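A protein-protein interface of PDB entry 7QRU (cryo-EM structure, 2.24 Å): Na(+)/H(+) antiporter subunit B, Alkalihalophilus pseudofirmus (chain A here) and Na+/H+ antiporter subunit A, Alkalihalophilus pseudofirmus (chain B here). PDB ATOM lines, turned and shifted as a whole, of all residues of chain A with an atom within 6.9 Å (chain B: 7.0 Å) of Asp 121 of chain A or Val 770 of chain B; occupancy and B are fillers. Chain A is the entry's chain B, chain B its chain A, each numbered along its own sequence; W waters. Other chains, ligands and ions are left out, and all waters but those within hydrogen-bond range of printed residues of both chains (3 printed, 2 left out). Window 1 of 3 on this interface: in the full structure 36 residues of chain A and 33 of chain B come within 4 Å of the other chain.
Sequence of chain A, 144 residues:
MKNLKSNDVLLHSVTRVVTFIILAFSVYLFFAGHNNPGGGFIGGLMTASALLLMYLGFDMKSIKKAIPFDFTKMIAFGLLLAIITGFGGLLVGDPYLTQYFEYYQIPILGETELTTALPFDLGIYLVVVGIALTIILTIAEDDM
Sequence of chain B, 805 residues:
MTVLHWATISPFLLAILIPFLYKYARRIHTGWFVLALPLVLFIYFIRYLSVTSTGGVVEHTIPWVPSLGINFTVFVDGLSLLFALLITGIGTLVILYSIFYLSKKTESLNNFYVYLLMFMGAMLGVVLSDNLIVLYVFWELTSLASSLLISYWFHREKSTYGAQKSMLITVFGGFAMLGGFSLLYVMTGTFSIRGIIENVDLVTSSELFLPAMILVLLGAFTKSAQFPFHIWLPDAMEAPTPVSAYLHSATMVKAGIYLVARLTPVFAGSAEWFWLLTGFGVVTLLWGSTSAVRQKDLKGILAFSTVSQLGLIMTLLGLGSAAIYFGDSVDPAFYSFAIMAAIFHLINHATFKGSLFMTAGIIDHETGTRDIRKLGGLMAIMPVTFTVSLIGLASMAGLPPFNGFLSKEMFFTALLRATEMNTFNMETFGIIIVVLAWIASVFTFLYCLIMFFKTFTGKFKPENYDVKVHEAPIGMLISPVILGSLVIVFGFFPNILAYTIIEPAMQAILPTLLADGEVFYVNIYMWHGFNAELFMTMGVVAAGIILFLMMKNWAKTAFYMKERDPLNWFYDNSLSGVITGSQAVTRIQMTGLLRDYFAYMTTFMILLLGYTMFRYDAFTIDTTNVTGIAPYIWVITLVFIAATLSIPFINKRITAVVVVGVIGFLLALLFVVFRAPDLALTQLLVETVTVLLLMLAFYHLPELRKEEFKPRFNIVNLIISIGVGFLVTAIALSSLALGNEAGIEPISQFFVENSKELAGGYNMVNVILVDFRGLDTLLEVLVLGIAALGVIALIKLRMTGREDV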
ATOM      1  N   LEU A  29     -28.801  17.163 -16.524  1.00  0.00           N
ATOM      2  CA  LEU A  29     -29.024  17.322 -15.102  1.00  0.00           C
ATOM      3  C   LEU A  29     -27.707  17.541 -14.385  1.00  0.00           C
ATOM      4  O   LEU A  29     -27.593  18.540 -13.708  1.00  0.00           O
ATOM      5  CB  LEU A  29     -29.736  16.084 -14.570  1.00  0.00           C
ATOM      6  CG  LEU A  29     -31.226  16.052 -14.960  1.00  0.00           C
ATOM      7  CD1 LEU A  29     -31.811  14.700 -14.646  1.00  0.00           C
ATOM      8  CD2 LEU A  29     -31.955  17.174 -14.295  1.00  0.00           C
ATOM      9  N   PHE A  30     -26.658  16.781 -14.743  1.00  0.00           N
ATOM     10  CA  PHE A  30     -25.379  17.026 -14.132  1.00  0.00           C
ATOM     11  C   PHE A  30     -24.917  18.453 -14.415  1.00  0.00           C
ATOM     12  O   PHE A  30     -24.551  19.141 -13.503  1.00  0.00           O
ATOM     13  CB  PHE A  30     -24.375  16.011 -14.644  1.00  0.00           C
ATOM     14  CG  PHE A  30     -22.965  16.344 -14.248  1.00  0.00           C
ATOM     15  CD1 PHE A  30     -22.522  16.203 -12.928  1.00  0.00           C
ATOM     16  CD2 PHE A  30     -22.126  16.974 -15.150  1.00  0.00           C
ATOM     17  CE1 PHE A  30     -21.228  16.559 -12.591  1.00  0.00           C
ATOM     18  CE2 PHE A  30     -20.842  17.371 -14.794  1.00  0.00           C
ATOM     19  CZ  PHE A  30     -20.365  17.105 -13.541  1.00  0.00           C
ATOM     20  N   PHE A  31     -24.855  18.922 -15.673  1.00  0.00           N
ATOM     21  CA  PHE A  31     -24.288  20.239 -15.897  1.00  0.00           C
ATOM     22  C   PHE A  31     -25.200  21.357 -15.412  1.00  0.00           C
ATOM     23  O   PHE A  31     -24.812  22.468 -15.453  1.00  0.00           O
ATOM     24  CB  PHE A  31     -24.022  20.458 -17.381  1.00  0.00           C
ATOM     25  CG  PHE A  31     -22.768  19.784 -17.808  1.00  0.00           C
ATOM     26  CD1 PHE A  31     -21.551  20.295 -17.420  1.00  0.00           C
ATOM     27  CD2 PHE A  31     -22.805  18.563 -18.452  1.00  0.00           C
ATOM     28  CE1 PHE A  31     -20.383  19.647 -17.787  1.00  0.00           C
ATOM     29  CE2 PHE A  31     -21.643  17.904 -18.810  1.00  0.00           C
ATOM     30  CZ  PHE A  31     -20.436  18.450 -18.469  1.00  0.00           C
ATOM     31  N   GLY A  33     -26.876  21.669 -12.615  1.00  0.00           N
ATOM     32  CA  GLY A  33     -26.949  21.790 -11.184  1.00  0.00           C
ATOM     33  C   GLY A  33     -26.619  23.175 -10.611  1.00  0.00           C
ATOM     34  O   GLY A  33     -27.293  23.627  -9.708  1.00  0.00           O
ATOM     35  N   HIS A  34     -25.627  23.862 -11.128  1.00  0.00           N
ATOM     36  CA  HIS A  34     -25.211  25.103 -10.517  1.00  0.00           C
ATOM     37  C   HIS A  34     -26.307  26.138 -10.640  1.00  0.00           C
ATOM     38  O   HIS A  34     -26.343  27.032  -9.801  1.00  0.00           O
ATOM     39  CB  HIS A  34     -23.877  25.585 -11.099  1.00  0.00           C
ATOM     40  CG  HIS A  34     -22.968  26.116 -10.040  1.00  0.00           C
ATOM     41  ND1 HIS A  34     -22.638  25.391  -8.882  1.00  0.00           N
ATOM     42  CD2 HIS A  34     -22.413  27.367  -9.924  1.00  0.00           C
ATOM     43  CE1 HIS A  34     -21.887  26.180  -8.081  1.00  0.00           C
ATOM     44  NE2 HIS A  34     -21.752  27.417  -8.713  1.00  0.00           N
ATOM     45  N   GLY A  38     -30.644  19.797 -10.473  1.00  0.00           N
ATOM     46  CA  GLY A  38     -29.742  18.798 -11.004  1.00  0.00           C
ATOM     47  C   GLY A  38     -28.470  18.669 -10.148  1.00  0.00           C
ATOM     48  O   GLY A  38     -28.495  18.945  -8.961  1.00  0.00           O
ATOM     49  N   GLY A  39     -27.320  18.431 -10.755  1.00  0.00           N
ATOM     50  CA  GLY A  39     -26.069  18.274 -10.035  1.00  0.00           C
ATOM     51  C   GLY A  39     -25.588  16.821 -10.061  1.00  0.00           C
ATOM     52  O   GLY A  39     -26.263  15.991 -10.633  1.00  0.00           O
ATOM     53  N   GLY A  40     -24.574  16.497  -9.251  1.00  0.00           N
ATOM     54  CA  GLY A  40     -23.924  15.218  -9.271  1.00  0.00           C
ATOM     55  C   GLY A  40     -24.838  14.074  -8.838  1.00  0.00           C
ATOM     56  O   GLY A  40     -24.789  13.010  -9.459  1.00  0.00           O
ATOM     57  N   PHE A  41     -25.553  14.243  -7.715  1.00  0.00           N
ATOM     58  CA  PHE A  41     -26.407  13.192  -7.206  1.00  0.00           C
ATOM     59  C   PHE A  41     -27.529  12.856  -8.194  1.00  0.00           C
ATOM     60  O   PHE A  41     -27.692  11.708  -8.634  1.00  0.00           O
ATOM     61  CB  PHE A  41     -26.960  13.654  -5.870  1.00  0.00           C
ATOM     62  CG  PHE A  41     -25.938  13.758  -4.771  1.00  0.00           C
ATOM     63  CD1 PHE A  41     -25.280  12.611  -4.308  1.00  0.00           C
ATOM     64  CD2 PHE A  41     -25.645  15.000  -4.205  1.00  0.00           C
ATOM     65  CE1 PHE A  41     -24.383  12.708  -3.268  1.00  0.00           C
ATOM     66  CE2 PHE A  41     -24.714  15.089  -3.181  1.00  0.00           C
ATOM     67  CZ  PHE A  41     -24.092  13.949  -2.717  1.00  0.00           C
ATOM     68  N   LEU A  81     -11.100  12.265  -7.239  1.00  0.00           N
ATOM     69  CA  LEU A  81     -11.307  13.510  -7.946  1.00  0.00           C
ATOM     70  C   LEU A  81     -11.931  14.572  -7.042  1.00  0.00           C
ATOM     71  O   LEU A  81     -11.439  15.683  -6.921  1.00  0.00           O
ATOM     72  CB  LEU A  81     -12.161  13.246  -9.161  1.00  0.00           C
ATOM     73  CG  LEU A  81     -12.525  14.507  -9.915  1.00  0.00           C
ATOM     74  CD1 LEU A  81     -11.281  15.289 -10.336  1.00  0.00           C
ATOM     75  CD2 LEU A  81     -13.320  14.096 -11.152  1.00  0.00           C
ATOM     76  N   ALA A  82     -12.900  14.161  -6.231  1.00  0.00           N
ATOM     77  CA  ALA A  82     -13.527  15.110  -5.336  1.00  0.00           C
ATOM     78  C   ALA A  82     -12.593  15.563  -4.229  1.00  0.00           C
ATOM     79  O   ALA A  82     -12.544  16.756  -3.936  1.00  0.00           O
ATOM     80  CB  ALA A  82     -14.814  14.479  -4.840  1.00  0.00           C
ATOM     81  N   THR A  85      -9.796  18.069  -5.882  1.00  0.00           N
ATOM     82  CA  THR A  85     -10.371  19.365  -6.203  1.00  0.00           C
ATOM     83  C   THR A  85     -10.351  20.303  -4.982  1.00  0.00           C
ATOM     84  O   THR A  85     -10.076  21.500  -5.084  1.00  0.00           O
ATOM     85  CB  THR A  85     -11.794  19.199  -6.758  1.00  0.00           C
ATOM     86  OG1 THR A  85     -11.709  18.513  -7.990  1.00  0.00           O
ATOM     87  CG2 THR A  85     -12.493  20.516  -6.966  1.00  0.00           C
ATOM     88  N   LEU A  97     -11.137  22.982   0.485  1.00  0.00           N
ATOM     89  CA  LEU A  97     -12.449  22.973  -0.094  1.00  0.00           C
ATOM     90  C   LEU A  97     -12.910  24.387  -0.414  1.00  0.00           C
ATOM     91  O   LEU A  97     -14.096  24.605  -0.478  1.00  0.00           O
ATOM     92  CB  LEU A  97     -13.388  22.208   0.847  1.00  0.00           C
ATOM     93  CG  LEU A  97     -13.808  20.853   0.250  1.00  0.00           C
ATOM     94  CD1 LEU A  97     -14.702  20.075   1.182  1.00  0.00           C
ATOM     95  CD2 LEU A  97     -14.539  21.072  -1.030  1.00  0.00           C
ATOM     96  N   GLN A  99     -13.696  26.993  -3.208  1.00  0.00           N
ATOM     97  CA  GLN A  99     -14.155  26.785  -4.594  1.00  0.00           C
ATOM     98  C   GLN A  99     -13.906  28.121  -5.269  1.00  0.00           C
ATOM     99  O   GLN A  99     -13.843  29.138  -4.594  1.00  0.00           O
ATOM    100  CB  GLN A  99     -15.639  26.404  -4.680  1.00  0.00           C
ATOM    101  CG  GLN A  99     -16.084  25.084  -4.062  1.00  0.00           C
ATOM    102  CD  GLN A  99     -15.555  23.790  -4.653  1.00  0.00           C
ATOM    103  OE1 GLN A  99     -14.552  23.759  -5.359  1.00  0.00           O
ATOM    104  NE2 GLN A  99     -16.235  22.670  -4.380  1.00  0.00           N
ATOM    105  N   THR A 116     -14.255  25.409  -9.938  1.00  0.00           N
ATOM    106  CA  THR A 116     -13.765  24.127  -9.372  1.00  0.00           C
ATOM    107  C   THR A 116     -14.929  23.231  -8.969  1.00  0.00           C
ATOM    108  O   THR A 116     -14.816  22.028  -8.968  1.00  0.00           O
ATOM    109  CB  THR A 116     -12.915  24.446  -8.152  1.00  0.00           C
ATOM    110  OG1 THR A 116     -13.635  25.349  -7.260  1.00  0.00           O
ATOM    111  CG2 THR A 116     -11.706  25.189  -8.657  1.00  0.00           C
ATOM    112  N   ALA A 117     -16.096  23.846  -8.734  1.00  0.00           N
ATOM    113  CA  ALA A 117     -17.325  23.116  -8.446  1.00  0.00           C
ATOM    114  C   ALA A 117     -17.668  22.120  -9.551  1.00  0.00           C
ATOM    115  O   ALA A 117     -18.294  21.138  -9.257  1.00  0.00           O
ATOM    116  CB  ALA A 117     -18.455  24.074  -8.226  1.00  0.00           C
ATOM    117  N   LEU A 118     -17.285  22.335 -10.795  1.00  0.00           N
ATOM    118  CA  LEU A 118     -17.535  21.344 -11.827  1.00  0.00           C
ATOM    119  C   LEU A 118     -16.733  20.049 -11.624  1.00  0.00           C
ATOM    120  O   LEU A 118     -17.274  18.949 -11.753  1.00  0.00           O
ATOM    121  CB  LEU A 118     -17.215  21.898 -13.223  1.00  0.00           C
ATOM    122  CG  LEU A 118     -17.615  20.975 -14.373  1.00  0.00           C
ATOM    123  CD1 LEU A 118     -19.139  20.745 -14.418  1.00  0.00           C
ATOM    124  CD2 LEU A 118     -17.085  21.567 -15.655  1.00  0.00           C
ATOM    125  N   PRO A 119     -15.405  20.056 -11.515  1.00  0.00           N
ATOM    126  CA  PRO A 119     -14.715  18.809 -11.203  1.00  0.00           C
ATOM    127  C   PRO A 119     -15.139  18.266  -9.831  1.00  0.00           C
ATOM    128  O   PRO A 119     -15.114  17.070  -9.633  1.00  0.00           O
ATOM    129  CB  PRO A 119     -13.238  19.148 -11.185  1.00  0.00           C
ATOM    130  CG  PRO A 119     -13.209  20.655 -11.182  1.00  0.00           C
ATOM    131  CD  PRO A 119     -14.494  21.125 -11.866  1.00  0.00           C
ATOM    132  N   PHE A 120     -15.495  19.108  -8.877  1.00  0.00           N
ATOM    133  CA  PHE A 120     -15.876  18.542  -7.605  1.00  0.00           C
ATOM    134  C   PHE A 120     -17.138  17.727  -7.793  1.00  0.00           C
ATOM    135  O   PHE A 120     -17.250  16.599  -7.303  1.00  0.00           O
ATOM    136  CB  PHE A 120     -16.119  19.663  -6.595  1.00  0.00           C
ATOM    137  CG  PHE A 120     -16.615  19.161  -5.282  1.00  0.00           C
ATOM    138  CD1 PHE A 120     -15.746  18.598  -4.377  1.00  0.00           C
ATOM    139  CD2 PHE A 120     -17.969  19.165  -4.979  1.00  0.00           C
ATOM    140  CE1 PHE A 120     -16.198  18.150  -3.136  1.00  0.00           C
ATOM    141  CE2 PHE A 120     -18.399  18.761  -3.718  1.00  0.00           C
ATOM    142  CZ  PHE A 120     -17.501  18.269  -2.790  1.00  0.00           C
ATOM    143  N   ASP A 121     -18.100  18.342  -8.475  1.00  0.00           N
ATOM    144  CA  ASP A 121     -19.371  17.709  -8.719  1.00  0.00           C
ATOM    145  C   ASP A 121     -19.213  16.567  -9.711  1.00  0.00           C
ATOM    146  O   ASP A 121     -19.968  15.598  -9.665  1.00  0.00           O
ATOM    147  CB  ASP A 121     -20.399  18.751  -9.100  1.00  0.00           C
ATOM    148  CG  ASP A 121     -21.813  18.250  -8.864  1.00  0.00           C
ATOM    149  OD1 ASP A 121     -22.160  17.911  -7.682  1.00  0.00           O
ATOM    150  OD2 ASP A 121     -22.547  18.121  -9.896  1.00  0.00           O
ATOM    151  N   LEU A 122     -18.195  16.546 -10.541  1.00  0.00           N
ATOM    152  CA  LEU A 122     -17.955  15.357 -11.381  1.00  0.00           C
ATOM    153  C   LEU A 122     -17.484  14.166 -10.549  1.00  0.00           C
ATOM    154  O   LEU A 122     -17.791  12.977 -10.868  1.00  0.00           O
ATOM    155  CB  LEU A 122     -16.945  15.694 -12.461  1.00  0.00           C
ATOM    156  CG  LEU A 122     -16.462  14.509 -13.276  1.00  0.00           C
ATOM    157  CD1 LEU A 122     -17.582  14.027 -14.141  1.00  0.00           C
ATOM    158  CD2 LEU A 122     -15.291  14.868 -14.127  1.00  0.00           C
ATOM    159  N   GLY A 123     -16.764  14.467  -9.460  1.00  0.00           N
ATOM    160  CA  GLY A 123     -16.324  13.388  -8.622  1.00  0.00           C
ATOM    161  C   GLY A 123     -17.557  12.795  -7.933  1.00  0.00           C
ATOM    162  O   GLY A 123     -17.701  11.579  -7.937  1.00  0.00           O
ATOM    163  N   ILE A 124     -18.461  13.637  -7.429  1.00  0.00           N
ATOM    164  CA  ILE A 124     -19.679  13.136  -6.803  1.00  0.00           C
ATOM    165  C   ILE A 124     -20.432  12.234  -7.793  1.00  0.00           C
ATOM    166  O   ILE A 124     -20.873  11.177  -7.430  1.00  0.00           O
ATOM    167  CB  ILE A 124     -20.613  14.270  -6.360  1.00  0.00           C
ATOM    168  CG1 ILE A 124     -19.962  15.266  -5.408  1.00  0.00           C
ATOM    169  CG2 ILE A 124     -21.987  13.730  -5.873  1.00  0.00           C
ATOM    170  CD1 ILE A 124     -18.966  14.657  -4.411  1.00  0.00           C
ATOM    171  N   TYR A 125     -20.645  12.730  -9.003  1.00  0.00           N
ATOM    172  CA  TYR A 125     -21.290  12.028 -10.078  1.00  0.00           C
ATOM    173  C   TYR A 125     -20.694  10.658 -10.340  1.00  0.00           C
ATOM    174  O   TYR A 125     -21.450   9.691 -10.453  1.00  0.00           O
ATOM    175  CB  TYR A 125     -21.255  12.918 -11.334  1.00  0.00           C
ATOM    176  CG  TYR A 125     -21.822  12.255 -12.539  1.00  0.00           C
ATOM    177  CD1 TYR A 125     -20.992  11.475 -13.322  1.00  0.00           C
ATOM    178  CD2 TYR A 125     -23.163  12.421 -12.930  1.00  0.00           C
ATOM    179  CE1 TYR A 125     -21.511  10.773 -14.397  1.00  0.00           C
ATOM    180  CE2 TYR A 125     -23.682  11.732 -14.031  1.00  0.00           C
ATOM    181  CZ  TYR A 125     -22.841  10.927 -14.777  1.00  0.00           C
ATOM    182  OH  TYR A 125     -23.201  10.156 -15.861  1.00  0.00           O
ATOM    183  N   LEU A 126     -19.365  10.530 -10.396  1.00  0.00           N
ATOM    184  CA  LEU A 126     -18.805   9.212 -10.657  1.00  0.00           C
ATOM    185  C   LEU A 126     -19.025   8.269  -9.509  1.00  0.00           C
ATOM    186  O   LEU A 126     -19.211   7.098  -9.720  1.00  0.00           O
ATOM    187  CB  LEU A 126     -17.296   9.343 -10.828  1.00  0.00           C
ATOM    188  CG  LEU A 126     -16.883  10.038 -12.135  1.00  0.00           C
ATOM    189  CD1 LEU A 126     -15.418  10.214 -12.149  1.00  0.00           C
ATOM    190  CD2 LEU A 126     -17.274   9.231 -13.342  1.00  0.00           C
ATOM    191  N   ALA B 759     -20.507  32.810  -5.035  1.00  0.00           N
ATOM    192  CA  ALA B 759     -20.252  31.403  -5.329  1.00  0.00           C
ATOM    193  C   ALA B 759     -20.683  31.078  -6.719  1.00  0.00           C
ATOM    194  O   ALA B 759     -20.587  29.941  -7.114  1.00  0.00           O
ATOM    195  CB  ALA B 759     -20.916  30.525  -4.304  1.00  0.00           C
ATOM    196  N   VAL B 765     -29.636  25.528  -3.484  1.00  0.00           N
ATOM    197  CA  VAL B 765     -29.408  24.280  -2.832  1.00  0.00           C
ATOM    198  C   VAL B 765     -28.092  23.699  -3.356  1.00  0.00           C
ATOM    199  O   VAL B 765     -27.272  23.296  -2.574  1.00  0.00           O
ATOM    200  CB  VAL B 765     -30.648  23.379  -3.013  1.00  0.00           C
ATOM    201  CG1 VAL B 765     -30.483  21.975  -2.522  1.00  0.00           C
ATOM    202  CG2 VAL B 765     -31.816  24.009  -2.306  1.00  0.00           C
ATOM    203  N   ASN B 766     -27.865  23.641  -4.664  1.00  0.00           N
ATOM    204  CA  ASN B 766     -26.616  23.078  -5.185  1.00  0.00           C
ATOM    205  C   ASN B 766     -25.415  23.863  -4.681  1.00  0.00           C
ATOM    206  O   ASN B 766     -24.406  23.263  -4.402  1.00  0.00           O
ATOM    207  CB  ASN B 766     -26.556  23.031  -6.707  1.00  0.00           C
ATOM    208  CG  ASN B 766     -25.469  22.108  -7.248  1.00  0.00           C
ATOM    209  OD1 ASN B 766     -25.604  20.887  -7.142  1.00  0.00           O
ATOM    210  ND2 ASN B 766     -24.402  22.691  -7.808  1.00  0.00           N
ATOM    211  N   VAL B 767     -25.531  25.181  -4.544  1.00  0.00           N
ATOM    212  CA  VAL B 767     -24.433  25.973  -4.116  1.00  0.00           C
ATOM    213  C   VAL B 767     -24.102  25.620  -2.667  1.00  0.00           C
ATOM    214  O   VAL B 767     -22.976  25.684  -2.246  1.00  0.00           O
ATOM    215  CB  VAL B 767     -24.736  27.439  -4.386  1.00  0.00           C
ATOM    216  CG1 VAL B 767     -23.730  28.330  -3.749  1.00  0.00           C
ATOM    217  CG2 VAL B 767     -24.779  27.681  -5.925  1.00  0.00           C
ATOM    218  N   ILE B 768     -25.106  25.376  -1.845  1.00  0.00           N
ATOM    219  CA  ILE B 768     -24.807  25.008  -0.507  1.00  0.00           C
ATOM    220  C   ILE B 768     -24.132  23.661  -0.509  1.00  0.00           C
ATOM    221  O   ILE B 768     -23.110  23.527   0.150  1.00  0.00           O
ATOM    222  CB  ILE B 768     -26.051  24.966   0.331  1.00  0.00           C
ATOM    223  CG1 ILE B 768     -26.544  26.389   0.573  1.00  0.00           C
ATOM    224  CG2 ILE B 768     -25.772  24.180   1.633  1.00  0.00           C
ATOM    225  CD1 ILE B 768     -28.014  26.329   1.058  1.00  0.00           C
ATOM    226  N   LEU B 769     -24.614  22.722  -1.323  1.00  0.00           N
ATOM    227  CA  LEU B 769     -24.013  21.424  -1.269  1.00  0.00           C
ATOM    228  C   LEU B 769     -22.563  21.435  -1.690  1.00  0.00           C
ATOM    229  O   LEU B 769     -21.929  20.486  -1.292  1.00  0.00           O
ATOM    230  CB  LEU B 769     -24.751  20.450  -2.172  1.00  0.00           C
ATOM    231  CG  LEU B 769     -26.175  20.136  -1.712  1.00  0.00           C
ATOM    232  CD1 LEU B 769     -26.833  19.247  -2.749  1.00  0.00           C
ATOM    233  CD2 LEU B 769     -26.156  19.478  -0.413  1.00  0.00           C
ATOM    234  N   VAL B 770     -22.159  22.157  -2.730  1.00  0.00           N
ATOM    235  CA  VAL B 770     -20.813  22.026  -3.269  1.00  0.00           C
ATOM    236  C   VAL B 770     -19.933  23.157  -2.749  1.00  0.00           C
ATOM    237  O   VAL B 770     -18.804  23.165  -3.080  1.00  0.00           O
ATOM    238  CB  VAL B 770     -20.727  22.046  -4.820  1.00  0.00           C
ATOM    239  CG1 VAL B 770     -21.516  20.941  -5.414  1.00  0.00           C
ATOM    240  CG2 VAL B 770     -21.166  23.360  -5.378  1.00  0.00           C
ATOM    241  N   ASP B 771     -20.456  24.217  -2.195  1.00  0.00           N
ATOM    242  CA  ASP B 771     -19.622  25.338  -1.850  1.00  0.00           C
ATOM    243  C   ASP B 771     -19.724  25.728  -0.368  1.00  0.00           C
ATOM    244  O   ASP B 771     -18.747  25.562   0.355  1.00  0.00           O
ATOM    245  CB  ASP B 771     -19.829  26.487  -2.807  1.00  0.00           C
ATOM    246  CG  ASP B 771     -18.726  27.499  -2.679  1.00  0.00           C
ATOM    247  OD1 ASP B 771     -18.073  27.519  -1.589  1.00  0.00           O
ATOM    248  OD2 ASP B 771     -18.477  28.231  -3.683  1.00  0.00           O
ATOM    249  N   PHE B 772     -20.855  26.183   0.138  1.00  0.00           N
ATOM    250  CA  PHE B 772     -20.886  26.631   1.525  1.00  0.00           C
ATOM    251  C   PHE B 772     -20.772  25.500   2.498  1.00  0.00           C
ATOM    252  O   PHE B 772     -20.147  25.745   3.493  1.00  0.00           O
ATOM    253  CB  PHE B 772     -22.148  27.385   1.832  1.00  0.00           C
ATOM    254  CG  PHE B 772     -22.274  28.629   0.985  1.00  0.00           C
ATOM    255  CD1 PHE B 772     -21.589  29.755   1.346  1.00  0.00           C
ATOM    256  CD2 PHE B 772     -23.280  28.750   0.019  1.00  0.00           C
ATOM    257  CE1 PHE B 772     -21.798  30.946   0.658  1.00  0.00           C
ATOM    258  CE2 PHE B 772     -23.525  29.957  -0.639  1.00  0.00           C
ATOM    259  CZ  PHE B 772     -22.703  31.017  -0.366  1.00  0.00           C
ATOM    260  N   ARG B 773     -21.113  24.265   2.095  1.00  0.00           N
ATOM    261  CA  ARG B 773     -21.177  23.139   2.989  1.00  0.00           C
ATOM    262  C   ARG B 773     -20.717  21.909   2.256  1.00  0.00           C
ATOM    263  O   ARG B 773     -21.293  20.818   2.413  1.00  0.00           O
ATOM    264  CB  ARG B 773     -22.583  22.861   3.616  1.00  0.00           C
ATOM    265  CG  ARG B 773     -23.027  24.038   4.506  1.00  0.00           C
ATOM    266  CD  ARG B 773     -24.308  23.735   5.242  1.00  0.00           C
ATOM    267  NE  ARG B 773     -24.290  22.443   5.908  1.00  0.00           N
ATOM    268  CZ  ARG B 773     -23.969  22.406   7.214  1.00  0.00           C
ATOM    269  NH1 ARG B 773     -23.859  23.545   7.907  1.00  0.00           N
ATOM    270  NH2 ARG B 773     -23.641  21.255   7.768  1.00  0.00           N
ATOM    271  N   GLY B 774     -19.685  22.103   1.464  1.00  0.00           N
ATOM    272  CA  GLY B 774     -19.171  21.080   0.574  1.00  0.00           C
ATOM    273  C   GLY B 774     -18.590  19.868   1.300  1.00  0.00           C
ATOM    274  O   GLY B 774     -18.668  18.730   0.793  1.00  0.00           O
ATOM    275  N   LEU B 775     -18.086  20.068   2.526  1.00  0.00           N
ATOM    276  CA  LEU B 775     -17.544  18.904   3.212  1.00  0.00           C
ATOM    277  C   LEU B 775     -18.596  17.817   3.463  1.00  0.00           C
ATOM    278  O   LEU B 775     -18.296  16.618   3.328  1.00  0.00           O
ATOM    279  CB  LEU B 775     -16.941  19.317   4.552  1.00  0.00           C
ATOM    280  CG  LEU B 775     -16.344  18.138   5.332  1.00  0.00           C
ATOM    281  CD1 LEU B 775     -15.216  17.622   4.523  1.00  0.00           C
ATOM    282  CD2 LEU B 775     -15.848  18.595   6.699  1.00  0.00           C
ATOM    283  N   THR B 777     -21.068  17.080   1.585  1.00  0.00           N
ATOM    284  CA  THR B 777     -21.308  16.353   0.364  1.00  0.00           C
ATOM    285  C   THR B 777     -20.210  15.330   0.076  1.00  0.00           C
ATOM    286  O   THR B 777     -20.476  14.294  -0.511  1.00  0.00           O
ATOM    287  CB  THR B 777     -21.429  17.338  -0.796  1.00  0.00           C
ATOM    288  OG1 THR B 777     -22.482  18.185  -0.403  1.00  0.00           O
ATOM    289  CG2 THR B 777     -21.797  16.678  -2.092  1.00  0.00           C
HETATM  290  O   HOH W   1     -19.575  27.652  -6.154  1.00  0.00           O
HETATM  291  O   HOH W   2     -16.716  24.086   0.980  1.00  0.00           O
HETATM  292  O   HOH W   3     -15.542  28.011  -1.511  1.00  0.00           O
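His 34 of chain A touches Val 770 of chain B (CE1 to CG2, 3.97 Å).
Asn 766 of chain B touches Gly 38 of chain A.
CA of Gly 39 of chain A touches OD1 of Asn 766 of chain B, 3.9 Å away.
Leu 775 of chain B touches Leu 97 of chain A.
Val 770 of chain B touches Ala 117 of chain A.
Gly 774 of chain B touches Phe 120 of chain A (O to CZ, 3.8 Å).
Asp 121 of chain A touches Val 770 of chain B (OD1 to CG1, 3.8 Å).
O of Ala 759 of chain B lies within hydrogen-bond range of NE2 of His 34 of chain A, at 3.2 Å.
The side-chain amide nitrogen (ND2) of Asn 766 of chain B is in hydrogen-bond range of a ring nitrogen (ND1) of His 34 of chain A (3.4 Å).
The side-chain amide nitrogen of Gln 99 of chain A sits at hydrogen-bond distance from the backbone carbonyl oxygen of Val 770 of chain B, at 2.9 Å.
Of the 25 printed residues of chain A, 10 touch a printed residue of chain B.
Of the 13 printed residues of chain B, 8 touch a printed residue of chain A.
Among the printed residues, no Asp or Glu carboxylate lies within 4 Å of a Lys or Arg side-chain nitrogen of the other chain.
Water W3 bridges OD1 of Asp 771 of chain B and N of Gln 99 of chain A.
Water W2 lies within hydrogen-bond range of the backbone carbonyl oxygen (O) of Asp 771 of chain B (2.6 Å) and the backbone carbonyl oxygen (O) of Leu 97 of chain A (3.0 Å).
Water W1 lies within hydrogen-bond range of the backbone carbonyl oxygen (O) of Ala 759 of chain B, the side-chain carboxylate (OD2) of Asp 771 of chain B and a ring nitrogen (NE2) of His 34 of chain A.
Of chain B, only Val 770 (3.8 Å) comes within 4 Å of Asp 121 of chain A.
Of the printed residues of chain B, Phe 120 of chain A touches Val 770 and Gly 774.
Printed residues of chain A within 4 Å of Leu 775 of chain B: Leu 97.
Printed residues of chain B within 4 Å of Gly 33 of chain A: Asn 766 (3.1 Å).
Leu 126 of chain A touches none of the printed residues of chain B.
The nearest printed residue of chain B that does not touch Asp 121 of chain A is Asn 766 of chain B (4.6 Å).
The backbone carbonyl oxygen of Val 767 of chain B sits at hydrogen-bond distance from the backbone NH of Phe 772 of chain B (3.2 Å).
The side-chain hydroxyl (OG1) of Thr 777 of chain B sits at hydrogen-bond distance from the backbone carbonyl oxygen (O) of Leu 769 of chain B (2.5 Å).
The side-chain carboxylate of Asp 121 of chain A is in hydrogen-bond range of the backbone NH of Gly 40 of chain A, 2.7 Å away.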
